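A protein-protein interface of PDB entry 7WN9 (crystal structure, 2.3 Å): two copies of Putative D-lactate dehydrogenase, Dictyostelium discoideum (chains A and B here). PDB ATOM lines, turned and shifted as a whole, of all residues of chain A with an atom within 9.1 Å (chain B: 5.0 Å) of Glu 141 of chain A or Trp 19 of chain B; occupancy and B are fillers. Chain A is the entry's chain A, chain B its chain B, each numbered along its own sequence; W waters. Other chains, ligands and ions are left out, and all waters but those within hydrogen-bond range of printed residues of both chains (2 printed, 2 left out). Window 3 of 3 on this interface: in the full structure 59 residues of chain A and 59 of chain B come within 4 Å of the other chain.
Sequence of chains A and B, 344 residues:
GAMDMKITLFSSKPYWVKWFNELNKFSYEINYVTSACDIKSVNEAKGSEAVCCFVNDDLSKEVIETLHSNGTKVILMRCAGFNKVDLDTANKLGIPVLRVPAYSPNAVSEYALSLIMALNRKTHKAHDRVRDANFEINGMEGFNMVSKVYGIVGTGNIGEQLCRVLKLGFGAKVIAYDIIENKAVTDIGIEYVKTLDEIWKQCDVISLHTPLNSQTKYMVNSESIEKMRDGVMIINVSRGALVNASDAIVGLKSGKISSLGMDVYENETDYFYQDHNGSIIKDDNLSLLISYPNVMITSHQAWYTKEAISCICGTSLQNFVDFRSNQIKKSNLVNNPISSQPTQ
The side-chain amide oxygen (OD1) of Asn 120 of chain A lies within hydrogen-bond range of the backbone NH (N) of Phe 143 of chain A (2.8 Å).
O of Glu 141 of chain A lies within hydrogen-bond range of NZ of Lys 122 of chain A (3.3 Å).
The guanidinium group (NH1) of Arg 129 of chain A lies within hydrogen-bond range of the backbone carbonyl oxygen (O) of Asn 138 of chain A, at 2.7 Å.
Of the printed residues of chain B, Glu 141 of chain A touches Trp 19, Tyr 304 and Lys 306.
Of chain A, only Glu 141 comes within 4 Å of Trp 19 of chain B.
Printed residues of chain A within 4 Å of Tyr 304 of chain B: Arg 121, Ile 137, Asn 138, Met 140, Glu 141 and Gly 142.
Of the printed residues of chain A, Lys 306 of chain B touches Glu 141 and Gly 142.
Ile 309 of chain B touches none of the printed residues of chain A.
The nearest residue of chain A that does not touch Trp 19 of chain B is Gly 142 of chain A (7.8 Å).
Printed residues of chain B that touch a printed residue of chain A: Tyr 15, Trp 19, Tyr 304, Thr 305 and Lys 306.
Along chain B the printed residues that touch a printed residue of chain A span positions 15 to 306.
Hydrophobic or aromatic side chains of chain A within 4 Å of the printed part of chain B: Ile 137.
Among the printed residues, no Asp or Glu carboxylate lies within 4 Å of a Lys or Arg side-chain nitrogen of the other chain.
OE1 of Glu 141 of chain A is in hydrogen-bond range of NE1 of Trp 19 of chain B (3.1 Å).
The backbone NH (N) of Gly 142 of chain A is in hydrogen-bond range of the backbone carbonyl oxygen (O) of Tyr 304 of chain B, 2.9 Å away.
O of Gly 142 of chain A lies within hydrogen-bond range of N of Lys 306 of chain B (3.0 Å).
OD1 of Asn 144 of chain A sits at hydrogen-bond distance from OG1 of Thr 305 of chain B (2.8 Å).
No position is printed for both chains.
Of the 15 pairs that touch across the chains among the printed residues, none has its exchanged pair printed and touching as well.
Arg 121 of chain A touches Tyr 304 of chain B (NH1 to N, 3.8 Å).
Thr 305 of chain B touches Arg 121 of chain A.
CG1 of Ile 137 of chain A touches OH of Tyr 15 of chain B, 3.5 Å away.
Tyr 304 of chain B touches Ile 137 of chain A (CE2 to O, 3.3 Å).
Asn 138 of chain A touches Tyr 15 of chain B (OD1 to CD2, 3.3 Å).
OH of Tyr 304 of chain B touches OD1 of Asn 138 of chain A, at 3.997 Å.
N of Glu 141 of chain A touches CE2 of Tyr 304 of chain B, 3.3 Å away.
CB of Lys 306 of chain B touches OE2 of Glu 141 of chain A, at 3.6 Å.
Gly 142 of chain A touches Thr 305 of chain B.
C of Phe 143 of chain A touches CG2 of Thr 305 of chain B, at 3.7 Å.
Water W1 lies within hydrogen-bond range of the side-chain carboxylate of Glu 141 of chain A (2.6 Å) and the side-chain hydroxyl of Tyr 304 of chain B (2.8 Å).
Water W2 lies within hydrogen-bond range of NZ of Lys 18 of chain B and OE2 of Glu 141 of chain A.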
ATOM      1  N   MET A 117      -2.768  32.063  17.376  1.00  0.00           N
ATOM      2  CA  MET A 117      -3.460  31.186  16.431  1.00  0.00           C
ATOM      3  C   MET A 117      -3.278  29.722  16.805  1.00  0.00           C
ATOM      4  O   MET A 117      -4.205  28.920  16.681  1.00  0.00           O
ATOM      5  CB  MET A 117      -2.953  31.435  15.009  1.00  0.00           C
ATOM      6  CG  MET A 117      -3.055  32.874  14.560  1.00  0.00           C
ATOM      7  SD  MET A 117      -4.697  33.551  14.848  1.00  0.00           S
ATOM      8  CE  MET A 117      -5.700  32.375  13.926  1.00  0.00           C
ATOM      9  N   ALA A 118      -2.086  29.362  17.277  1.00  0.00           N
ATOM     10  CA  ALA A 118      -1.851  27.994  17.709  1.00  0.00           C
ATOM     11  C   ALA A 118      -2.740  27.643  18.894  1.00  0.00           C
ATOM     12  O   ALA A 118      -3.396  26.597  18.899  1.00  0.00           O
ATOM     13  CB  ALA A 118      -0.371  27.796  18.060  1.00  0.00           C
ATOM     14  N   LEU A 119      -2.753  28.493  19.930  1.00  0.00           N
ATOM     15  CA  LEU A 119      -3.575  28.190  21.100  1.00  0.00           C
ATOM     16  C   LEU A 119      -5.058  28.318  20.798  1.00  0.00           C
ATOM     17  O   LEU A 119      -5.881  27.727  21.501  1.00  0.00           O
ATOM     18  CB  LEU A 119      -3.222  29.110  22.263  1.00  0.00           C
ATOM     19  CG  LEU A 119      -1.798  28.985  22.804  1.00  0.00           C
ATOM     20  CD1 LEU A 119      -1.502  30.156  23.724  1.00  0.00           C
ATOM     21  CD2 LEU A 119      -1.586  27.651  23.538  1.00  0.00           C
ATOM     22  N   ASN A 120      -5.413  29.096  19.781  1.00  0.00           N
ATOM     23  CA  ASN A 120      -6.810  29.268  19.399  1.00  0.00           C
ATOM     24  C   ASN A 120      -7.286  28.058  18.593  1.00  0.00           C
ATOM     25  O   ASN A 120      -8.117  27.276  19.059  1.00  0.00           O
ATOM     26  CB  ASN A 120      -6.955  30.578  18.612  1.00  0.00           C
ATOM     27  CG  ASN A 120      -8.333  30.770  18.011  1.00  0.00           C
ATOM     28  OD1 ASN A 120      -9.247  29.974  18.224  1.00  0.00           O
ATOM     29  ND2 ASN A 120      -8.489  31.855  17.261  1.00  0.00           N
ATOM     30  N   ARG A 121      -6.725  27.865  17.397  1.00  0.00           N
ATOM     31  CA  ARG A 121      -7.162  26.796  16.506  1.00  0.00           C
ATOM     32  C   ARG A 121      -6.472  25.459  16.773  1.00  0.00           C
ATOM     33  O   ARG A 121      -6.897  24.447  16.208  1.00  0.00           O
ATOM     34  CB  ARG A 121      -6.963  27.222  15.043  1.00  0.00           C
ATOM     35  CG  ARG A 121      -7.647  28.578  14.695  1.00  0.00           C
ATOM     36  CD  ARG A 121      -9.137  28.629  15.144  1.00  0.00           C
ATOM     37  NE  ARG A 121      -9.914  27.548  14.537  1.00  0.00           N
ATOM     38  CZ  ARG A 121     -10.549  27.656  13.369  1.00  0.00           C
ATOM     39  NH1 ARG A 121     -11.196  26.623  12.864  1.00  0.00           N
ATOM     40  NH2 ARG A 121     -10.524  28.797  12.696  1.00  0.00           N
ATOM     41  N   LYS A 122      -5.434  25.427  17.610  1.00  0.00           N
ATOM     42  CA  LYS A 122      -4.833  24.173  18.096  1.00  0.00           C
ATOM     43  C   LYS A 122      -4.250  23.320  16.968  1.00  0.00           C
ATOM     44  O   LYS A 122      -4.342  22.088  16.984  1.00  0.00           O
ATOM     45  CB  LYS A 122      -5.854  23.378  18.917  1.00  0.00           C
ATOM     46  CG  LYS A 122      -6.415  24.240  20.020  1.00  0.00           C
ATOM     47  CD  LYS A 122      -7.336  23.526  20.941  1.00  0.00           C
ATOM     48  CE  LYS A 122      -7.908  24.522  21.923  1.00  0.00           C
ATOM     49  NZ  LYS A 122      -8.496  25.675  21.188  1.00  0.00           N
ATOM     50  N   LYS A 125      -1.909  20.639  18.370  1.00  0.00           N
ATOM     51  CA  LYS A 125      -2.648  19.502  18.916  1.00  0.00           C
ATOM     52  C   LYS A 125      -3.219  18.625  17.806  1.00  0.00           C
ATOM     53  O   LYS A 125      -3.202  17.388  17.904  1.00  0.00           O
ATOM     54  CB  LYS A 125      -3.771  20.010  19.823  1.00  0.00           C
ATOM     55  CG  LYS A 125      -4.579  18.912  20.522  1.00  0.00           C
ATOM     56  CD  LYS A 125      -5.724  19.505  21.361  1.00  0.00           C
ATOM     57  CE  LYS A 125      -6.215  18.524  22.440  1.00  0.00           C
ATOM     58  NZ  LYS A 125      -5.283  18.391  23.630  1.00  0.00           N
ATOM     59  N   ARG A 129      -2.272  14.662  17.049  1.00  0.00           N
ATOM     60  CA  ARG A 129      -3.295  13.627  16.918  1.00  0.00           C
ATOM     61  C   ARG A 129      -3.175  12.901  15.586  1.00  0.00           C
ATOM     62  O   ARG A 129      -3.185  11.665  15.533  1.00  0.00           O
ATOM     63  CB  ARG A 129      -4.688  14.230  17.065  1.00  0.00           C
ATOM     64  CG  ARG A 129      -5.106  14.505  18.513  1.00  0.00           C
ATOM     65  CD  ARG A 129      -6.602  14.842  18.578  1.00  0.00           C
ATOM     66  NE  ARG A 129      -6.970  15.294  19.915  1.00  0.00           N
ATOM     67  CZ  ARG A 129      -8.169  15.751  20.258  1.00  0.00           C
ATOM     68  NH1 ARG A 129      -9.146  15.831  19.358  1.00  0.00           N
ATOM     69  NH2 ARG A 129      -8.387  16.135  21.505  1.00  0.00           N
ATOM     70  N   ILE A 137     -11.608  15.463  16.282  1.00  0.00           N
ATOM     71  CA  ILE A 137     -11.418  16.903  16.445  1.00  0.00           C
ATOM     72  C   ILE A 137     -12.084  17.450  17.688  1.00  0.00           C
ATOM     73  O   ILE A 137     -11.964  18.655  17.944  1.00  0.00           O
ATOM     74  CB  ILE A 137     -11.889  17.693  15.208  1.00  0.00           C
ATOM     75  CG1 ILE A 137     -13.415  17.606  15.059  1.00  0.00           C
ATOM     76  CG2 ILE A 137     -11.164  17.184  13.965  1.00  0.00           C
ATOM     77  CD1 ILE A 137     -13.999  18.566  14.003  1.00  0.00           C
ATOM     78  N   ASN A 138     -12.767  16.618  18.479  1.00  0.00           N
ATOM     79  CA  ASN A 138     -13.290  17.092  19.755  1.00  0.00           C
ATOM     80  C   ASN A 138     -12.158  17.674  20.597  1.00  0.00           C
ATOM     81  O   ASN A 138     -11.060  17.113  20.669  1.00  0.00           O
ATOM     82  CB  ASN A 138     -13.990  15.959  20.524  1.00  0.00           C
ATOM     83  CG  ASN A 138     -14.912  16.485  21.624  1.00  0.00           C
ATOM     84  OD1 ASN A 138     -15.661  17.464  21.426  1.00  0.00           O
ATOM     85  ND2 ASN A 138     -14.860  15.849  22.792  1.00  0.00           N
ATOM     86  N   GLY A 139     -12.427  18.808  21.241  1.00  0.00           N
ATOM     87  CA  GLY A 139     -11.402  19.530  21.969  1.00  0.00           C
ATOM     88  C   GLY A 139     -10.690  20.604  21.175  1.00  0.00           C
ATOM     89  O   GLY A 139      -9.821  21.286  21.727  1.00  0.00           O
ATOM     90  N   MET A 140     -11.031  20.796  19.903  1.00  0.00           N
ATOM     91  CA  MET A 140     -10.322  21.768  19.082  1.00  0.00           C
ATOM     92  C   MET A 140     -11.173  22.967  18.710  1.00  0.00           C
ATOM     93  O   MET A 140     -10.819  23.697  17.778  1.00  0.00           O
ATOM     94  CB  MET A 140      -9.796  21.098  17.822  1.00  0.00           C
ATOM     95  CG  MET A 140      -9.108  19.821  18.162  1.00  0.00           C
ATOM     96  SD  MET A 140      -7.405  19.836  17.656  1.00  0.00           S
ATOM     97  CE  MET A 140      -7.368  18.257  16.839  1.00  0.00           C
ATOM     98  N   GLU A 141     -12.272  23.196  19.417  1.00  0.00           N
ATOM     99  CA  GLU A 141     -13.094  24.362  19.123  1.00  0.00           C
ATOM    100  C   GLU A 141     -12.289  25.650  19.288  1.00  0.00           C
ATOM    101  O   GLU A 141     -11.723  25.908  20.348  1.00  0.00           O
ATOM    102  CB  GLU A 141     -14.323  24.397  20.035  1.00  0.00           C
ATOM    103  CG  GLU A 141     -15.303  25.503  19.654  1.00  0.00           C
ATOM    104  CD  GLU A 141     -16.505  25.565  20.578  1.00  0.00           C
ATOM    105  OE1 GLU A 141     -17.393  24.688  20.473  1.00  0.00           O
ATOM    106  OE2 GLU A 141     -16.549  26.487  21.415  1.00  0.00           O
ATOM    107  N   GLY A 142     -12.260  26.472  18.244  1.00  0.00           N
ATOM    108  CA  GLY A 142     -11.599  27.754  18.291  1.00  0.00           C
ATOM    109  C   GLY A 142     -12.583  28.904  18.427  1.00  0.00           C
ATOM    110  O   GLY A 142     -13.760  28.726  18.744  1.00  0.00           O
ATOM    111  N   PHE A 143     -12.069  30.110  18.196  1.00  0.00           N
ATOM    112  CA  PHE A 143     -12.892  31.302  18.158  1.00  0.00           C
ATOM    113  C   PHE A 143     -12.544  32.089  16.903  1.00  0.00           C
ATOM    114  O   PHE A 143     -11.427  32.000  16.388  1.00  0.00           O
ATOM    115  CB  PHE A 143     -12.736  32.166  19.439  1.00  0.00           C
ATOM    116  CG  PHE A 143     -11.315  32.584  19.758  1.00  0.00           C
ATOM    117  CD1 PHE A 143     -10.764  33.732  19.191  1.00  0.00           C
ATOM    118  CD2 PHE A 143     -10.546  31.852  20.658  1.00  0.00           C
ATOM    119  CE1 PHE A 143      -9.457  34.136  19.505  1.00  0.00           C
ATOM    120  CE2 PHE A 143      -9.239  32.237  20.969  1.00  0.00           C
ATOM    121  CZ  PHE A 143      -8.693  33.385  20.392  1.00  0.00           C
ATOM    122  N   ASN A 144     -13.534  32.793  16.363  1.00  0.00           N
ATOM    123  CA  ASN A 144     -13.254  33.783  15.335  1.00  0.00           C
ATOM    124  C   ASN A 144     -12.484  34.930  15.964  1.00  0.00           C
ATOM    125  O   ASN A 144     -12.817  35.378  17.063  1.00  0.00           O
ATOM    126  CB  ASN A 144     -14.547  34.308  14.713  1.00  0.00           C
ATOM    127  CG  ASN A 144     -15.268  33.263  13.877  1.00  0.00           C
ATOM    128  OD1 ASN A 144     -14.862  32.099  13.811  1.00  0.00           O
ATOM    129  ND2 ASN A 144     -16.345  33.680  13.230  1.00  0.00           N
ATOM    130  N   LYS A 148     -12.997  38.341  20.099  1.00  0.00           N
ATOM    131  CA  LYS A 148     -12.311  38.625  21.353  1.00  0.00           C
ATOM    132  C   LYS A 148     -11.845  40.077  21.418  1.00  0.00           C
ATOM    133  O   LYS A 148     -11.573  40.706  20.388  1.00  0.00           O
ATOM    134  CB  LYS A 148     -11.106  37.691  21.535  1.00  0.00           C
ATOM    135  CG  LYS A 148     -11.451  36.205  21.516  1.00  0.00           C
ATOM    136  CD  LYS A 148     -12.424  35.852  22.618  1.00  0.00           C
ATOM    137  CE  LYS A 148     -12.572  34.333  22.767  1.00  0.00           C
ATOM    138  NZ  LYS A 148     -13.786  33.986  23.573  1.00  0.00           N
ATOM    139  N   MET A 233      -6.662  34.437  27.642  1.00  0.00           N
ATOM    140  CA  MET A 233      -5.459  33.940  26.994  1.00  0.00           C
ATOM    141  C   MET A 233      -4.333  34.956  27.191  1.00  0.00           C
ATOM    142  O   MET A 233      -4.522  36.159  26.951  1.00  0.00           O
ATOM    143  CB  MET A 233      -5.694  33.694  25.501  1.00  0.00           C
ATOM    144  CG  MET A 233      -4.412  33.301  24.724  1.00  0.00           C
ATOM    145  SD  MET A 233      -4.600  33.328  22.917  1.00  0.00           S
ATOM    146  CE  MET A 233      -5.733  31.946  22.667  1.00  0.00           C
ATOM    147  N   TYR B  15     -19.474  17.372  20.429  1.00  0.00           N
ATOM    148  CA  TYR B  15     -19.716  18.769  20.080  1.00  0.00           C
ATOM    149  C   TYR B  15     -21.046  18.954  19.342  1.00  0.00           C
ATOM    150  O   TYR B  15     -21.667  20.014  19.461  1.00  0.00           O
ATOM    151  CB  TYR B  15     -18.550  19.344  19.263  1.00  0.00           C
ATOM    152  CG  TYR B  15     -18.024  18.462  18.151  1.00  0.00           C
ATOM    153  CD1 TYR B  15     -18.518  18.564  16.851  1.00  0.00           C
ATOM    154  CD2 TYR B  15     -17.012  17.542  18.397  1.00  0.00           C
ATOM    155  CE1 TYR B  15     -18.014  17.758  15.818  1.00  0.00           C
ATOM    156  CE2 TYR B  15     -16.512  16.732  17.384  1.00  0.00           C
ATOM    157  CZ  TYR B  15     -17.014  16.837  16.104  1.00  0.00           C
ATOM    158  OH  TYR B  15     -16.518  16.018  15.111  1.00  0.00           O
ATOM    159  N   TRP B  16     -21.506  17.957  18.582  1.00  0.00           N
ATOM    160  CA  TRP B  16     -22.840  18.062  17.998  1.00  0.00           C
ATOM    161  C   TRP B  16     -23.909  17.979  19.084  1.00  0.00           C
ATOM    162  O   TRP B  16     -24.853  18.780  19.103  1.00  0.00           O
ATOM    163  CB  TRP B  16     -23.077  16.975  16.946  1.00  0.00           C
ATOM    164  CG  TRP B  16     -22.185  17.011  15.747  1.00  0.00           C
ATOM    165  CD1 TRP B  16     -21.438  15.978  15.271  1.00  0.00           C
ATOM    166  CD2 TRP B  16     -21.964  18.112  14.851  1.00  0.00           C
ATOM    167  NE1 TRP B  16     -20.753  16.362  14.149  1.00  0.00           N
ATOM    168  CE2 TRP B  16     -21.052  17.669  13.869  1.00  0.00           C
ATOM    169  CE3 TRP B  16     -22.431  19.424  14.792  1.00  0.00           C
ATOM    170  CZ2 TRP B  16     -20.605  18.492  12.834  1.00  0.00           C
ATOM    171  CZ3 TRP B  16     -21.989  20.247  13.756  1.00  0.00           C
ATOM    172  CH2 TRP B  16     -21.082  19.778  12.797  1.00  0.00           C
ATOM    173  N   VAL B  17     -23.771  17.020  20.003  1.00  0.00           N
ATOM    174  CA  VAL B  17     -24.723  16.918  21.108  1.00  0.00           C
ATOM    175  C   VAL B  17     -24.821  18.246  21.838  1.00  0.00           C
ATOM    176  O   VAL B  17     -25.912  18.781  22.062  1.00  0.00           O
ATOM    177  CB  VAL B  17     -24.322  15.793  22.075  1.00  0.00           C
ATOM    178  CG1 VAL B  17     -25.256  15.823  23.288  1.00  0.00           C
ATOM    179  CG2 VAL B  17     -24.379  14.447  21.392  1.00  0.00           C
ATOM    180  N   LYS B  18     -23.671  18.797  22.217  1.00  0.00           N
ATOM    181  CA  LYS B  18     -23.656  20.030  22.989  1.00  0.00           C
ATOM    182  C   LYS B  18     -24.403  21.146  22.263  1.00  0.00           C
ATOM    183  O   LYS B  18     -25.248  21.828  22.849  1.00  0.00           O
ATOM    184  CB  LYS B  18     -22.208  20.424  23.269  1.00  0.00           C
ATOM    185  CG  LYS B  18     -22.047  21.544  24.281  1.00  0.00           C
ATOM    186  CD  LYS B  18     -22.065  22.915  23.627  1.00  0.00           C
ATOM    187  CE  LYS B  18     -21.592  23.976  24.618  1.00  0.00           C
ATOM    188  NZ  LYS B  18     -21.711  25.352  24.066  1.00  0.00           N
ATOM    189  N   TRP B  19     -24.111  21.338  20.976  1.00  0.00           N
ATOM    190  CA  TRP B  19     -24.631  22.508  20.281  1.00  0.00           C
ATOM    191  C   TRP B  19     -26.072  22.328  19.830  1.00  0.00           C
ATOM    192  O   TRP B  19     -26.848  23.286  19.884  1.00  0.00           O
ATOM    193  CB  TRP B  19     -23.727  22.855  19.105  1.00  0.00           C
ATOM    194  CG  TRP B  19     -22.559  23.641  19.601  1.00  0.00           C
ATOM    195  CD1 TRP B  19     -21.274  23.203  19.769  1.00  0.00           C
ATOM    196  CD2 TRP B  19     -22.584  24.993  20.051  1.00  0.00           C
ATOM    197  NE1 TRP B  19     -20.500  24.207  20.279  1.00  0.00           N
ATOM    198  CE2 TRP B  19     -21.280  25.319  20.464  1.00  0.00           C
ATOM    199  CE3 TRP B  19     -23.590  25.968  20.143  1.00  0.00           C
ATOM    200  CZ2 TRP B  19     -20.946  26.583  20.952  1.00  0.00           C
ATOM    201  CZ3 TRP B  19     -23.261  27.222  20.628  1.00  0.00           C
ATOM    202  CH2 TRP B  19     -21.953  27.518  21.031  1.00  0.00           C
ATOM    203  N   PHE B  20     -26.458  21.119  19.390  1.00  0.00           N
ATOM    204  CA  PHE B  20     -27.859  20.902  19.034  1.00  0.00           C
ATOM    205  C   PHE B  20     -28.756  20.975  20.265  1.00  0.00           C
ATOM    206  O   PHE B  20     -29.868  21.502  20.191  1.00  0.00           O
ATOM    207  CB  PHE B  20     -28.040  19.567  18.302  1.00  0.00           C
ATOM    208  CG  PHE B  20     -27.820  19.659  16.807  1.00  0.00           C
ATOM    209  CD1 PHE B  20     -28.884  19.874  15.952  1.00  0.00           C
ATOM    210  CD2 PHE B  20     -26.546  19.538  16.265  1.00  0.00           C
ATOM    211  CE1 PHE B  20     -28.686  19.963  14.572  1.00  0.00           C
ATOM    212  CE2 PHE B  20     -26.341  19.623  14.897  1.00  0.00           C
ATOM    213  CZ  PHE B  20     -27.412  19.840  14.047  1.00  0.00           C
ATOM    214  N   ASN B  21     -28.287  20.469  21.412  1.00  0.00           N
ATOM    215  CA  ASN B  21     -29.075  20.579  22.638  1.00  0.00           C
ATOM    216  C   ASN B  21     -29.182  22.022  23.093  1.00  0.00           C
ATOM    217  O   ASN B  21     -30.251  22.465  23.525  1.00  0.00           O
ATOM    218  CB  ASN B  21     -28.470  19.741  23.757  1.00  0.00           C
ATOM    219  CG  ASN B  21     -28.801  18.290  23.626  1.00  0.00           C
ATOM    220  OD1 ASN B  21     -29.615  17.905  22.782  1.00  0.00           O
ATOM    221  ND2 ASN B  21     -28.172  17.461  24.456  1.00  0.00           N
ATOM    222  N   GLU B  22     -28.087  22.773  23.000  1.00  0.00           N
ATOM    223  CA  GLU B  22     -28.148  24.168  23.400  1.00  0.00           C
ATOM    224  C   GLU B  22     -29.143  24.948  22.549  1.00  0.00           C
ATOM    225  O   GLU B  22     -29.902  25.773  23.070  1.00  0.00           O
ATOM    226  CB  GLU B  22     -26.763  24.797  23.313  1.00  0.00           C
ATOM    227  CG  GLU B  22     -26.780  26.274  23.657  1.00  0.00           C
ATOM    228  CD  GLU B  22     -25.385  26.820  23.864  1.00  0.00           C
ATOM    229  OE1 GLU B  22     -24.422  26.017  23.831  1.00  0.00           O
ATOM    230  OE2 GLU B  22     -25.248  28.045  24.063  1.00  0.00           O
ATOM    231  N   LEU B  23     -29.163  24.701  21.242  1.00  0.00           N
ATOM    232  CA  LEU B  23     -29.955  25.518  20.331  1.00  0.00           C
ATOM    233  C   LEU B  23     -31.344  24.950  20.049  1.00  0.00           C
ATOM    234  O   LEU B  23     -32.129  25.599  19.351  1.00  0.00           O
ATOM    235  CB  LEU B  23     -29.196  25.712  19.013  1.00  0.00           C
ATOM    236  CG  LEU B  23     -27.866  26.460  19.166  1.00  0.00           C
ATOM    237  CD1 LEU B  23     -27.046  26.451  17.869  1.00  0.00           C
ATOM    238  CD2 LEU B  23     -28.134  27.874  19.643  1.00  0.00           C
ATOM    239  N   ASN B  24     -31.681  23.771  20.577  1.00  0.00           N
ATOM    240  CA  ASN B  24     -32.992  23.168  20.325  1.00  0.00           C
ATOM    241  C   ASN B  24     -34.010  23.790  21.279  1.00  0.00           C
ATOM    242  O   ASN B  24     -34.304  23.273  22.360  1.00  0.00           O
ATOM    243  CB  ASN B  24     -32.936  21.653  20.480  1.00  0.00           C
ATOM    244  CG  ASN B  24     -34.291  21.004  20.302  1.00  0.00           C
ATOM    245  OD1 ASN B  24     -35.239  21.645  19.823  1.00  0.00           O
ATOM    246  ND2 ASN B  24     -34.400  19.730  20.695  1.00  0.00           N
ATOM    247  N   TYR B 304     -14.552  24.829  12.655  1.00  0.00           N
ATOM    248  CA  TYR B 304     -14.859  24.486  14.045  1.00  0.00           C
ATOM    249  C   TYR B 304     -14.439  25.621  14.984  1.00  0.00           C
ATOM    250  O   TYR B 304     -13.488  25.520  15.759  1.00  0.00           O
ATOM    251  CB  TYR B 304     -14.189  23.166  14.420  1.00  0.00           C
ATOM    252  CG  TYR B 304     -14.598  22.582  15.759  1.00  0.00           C
ATOM    253  CD1 TYR B 304     -15.787  22.963  16.385  1.00  0.00           C
ATOM    254  CD2 TYR B 304     -13.792  21.646  16.406  1.00  0.00           C
ATOM    255  CE1 TYR B 304     -16.160  22.422  17.614  1.00  0.00           C
ATOM    256  CE2 TYR B 304     -14.161  21.097  17.639  1.00  0.00           C
ATOM    257  CZ  TYR B 304     -15.343  21.485  18.232  1.00  0.00           C
ATOM    258  OH  TYR B 304     -15.702  20.941  19.456  1.00  0.00           O
ATOM    259  N   THR B 305     -15.181  26.725  14.899  1.00  0.00           N
ATOM    260  CA  THR B 305     -15.163  27.743  15.939  1.00  0.00           C
ATOM    261  C   THR B 305     -16.532  27.800  16.604  1.00  0.00           C
ATOM    262  O   THR B 305     -17.531  27.296  16.079  1.00  0.00           O
ATOM    263  CB  THR B 305     -14.811  29.145  15.408  1.00  0.00           C
ATOM    264  OG1 THR B 305     -15.801  29.562  14.458  1.00  0.00           O
ATOM    265  CG2 THR B 305     -13.406  29.165  14.757  1.00  0.00           C
ATOM    266  N   LYS B 306     -16.558  28.446  17.768  1.00  0.00           N
ATOM    267  CA  LYS B 306     -17.808  28.653  18.486  1.00  0.00           C
ATOM    268  C   LYS B 306     -18.862  29.289  17.584  1.00  0.00           C
ATOM    269  O   LYS B 306     -19.968  28.761  17.432  1.00  0.00           O
ATOM    270  CB  LYS B 306     -17.539  29.512  19.722  1.00  0.00           C
ATOM    271  CG  LYS B 306     -18.694  29.619  20.700  1.00  0.00           C
ATOM    272  CD  LYS B 306     -18.297  30.455  21.912  1.00  0.00           C
ATOM    273  CE  LYS B 306     -19.518  30.824  22.761  1.00  0.00           C
ATOM    274  NZ  LYS B 306     -19.223  31.928  23.728  1.00  0.00           N
ATOM    275  N   ILE B 309     -19.802  26.797  14.378  1.00  0.00           N
ATOM    276  CA  ILE B 309     -20.550  25.577  14.656  1.00  0.00           C
ATOM    277  C   ILE B 309     -21.917  25.925  15.223  1.00  0.00           C
ATOM    278  O   ILE B 309     -22.888  25.184  15.033  1.00  0.00           O
ATOM    279  CB  ILE B 309     -19.755  24.640  15.593  1.00  0.00           C
ATOM    280  CG1 ILE B 309     -20.402  23.248  15.630  1.00  0.00           C
ATOM    281  CG2 ILE B 309     -19.659  25.225  17.024  1.00  0.00           C
ATOM    282  CD1 ILE B 309     -19.732  22.265  16.612  1.00  0.00           C
ATOM    283  N   SER B 310     -22.017  27.050  15.930  1.00  0.00           N
ATOM    284  CA  SER B 310     -23.321  27.548  16.345  1.00  0.00           C
ATOM    285  C   SER B 310     -24.221  27.822  15.137  1.00  0.00           C
ATOM    286  O   SER B 310     -25.416  27.506  15.160  1.00  0.00           O
ATOM    287  CB  SER B 310     -23.136  28.812  17.181  1.00  0.00           C
ATOM    288  OG  SER B 310     -24.377  29.321  17.606  1.00  0.00           O
ATOM    289  N   CYS B 313     -25.338  24.357  13.450  1.00  0.00           N
ATOM    290  CA  CYS B 313     -26.396  23.658  14.171  1.00  0.00           C
ATOM    291  C   CYS B 313     -27.685  24.466  14.177  1.00  0.00           C
ATOM    292  O   CYS B 313     -28.774  23.910  13.994  1.00  0.00           O
ATOM    293  CB  CYS B 313     -25.929  23.345  15.591  1.00  0.00           C
ATOM    294  SG  CYS B 313     -24.447  22.317  15.610  1.00  0.00           S
HETATM  295  O   HOH W   1     -17.664  22.206  21.001  1.00  0.00           O
HETATM  296  O   HOH W   2     -18.653  25.084  23.524  1.00  0.00           O
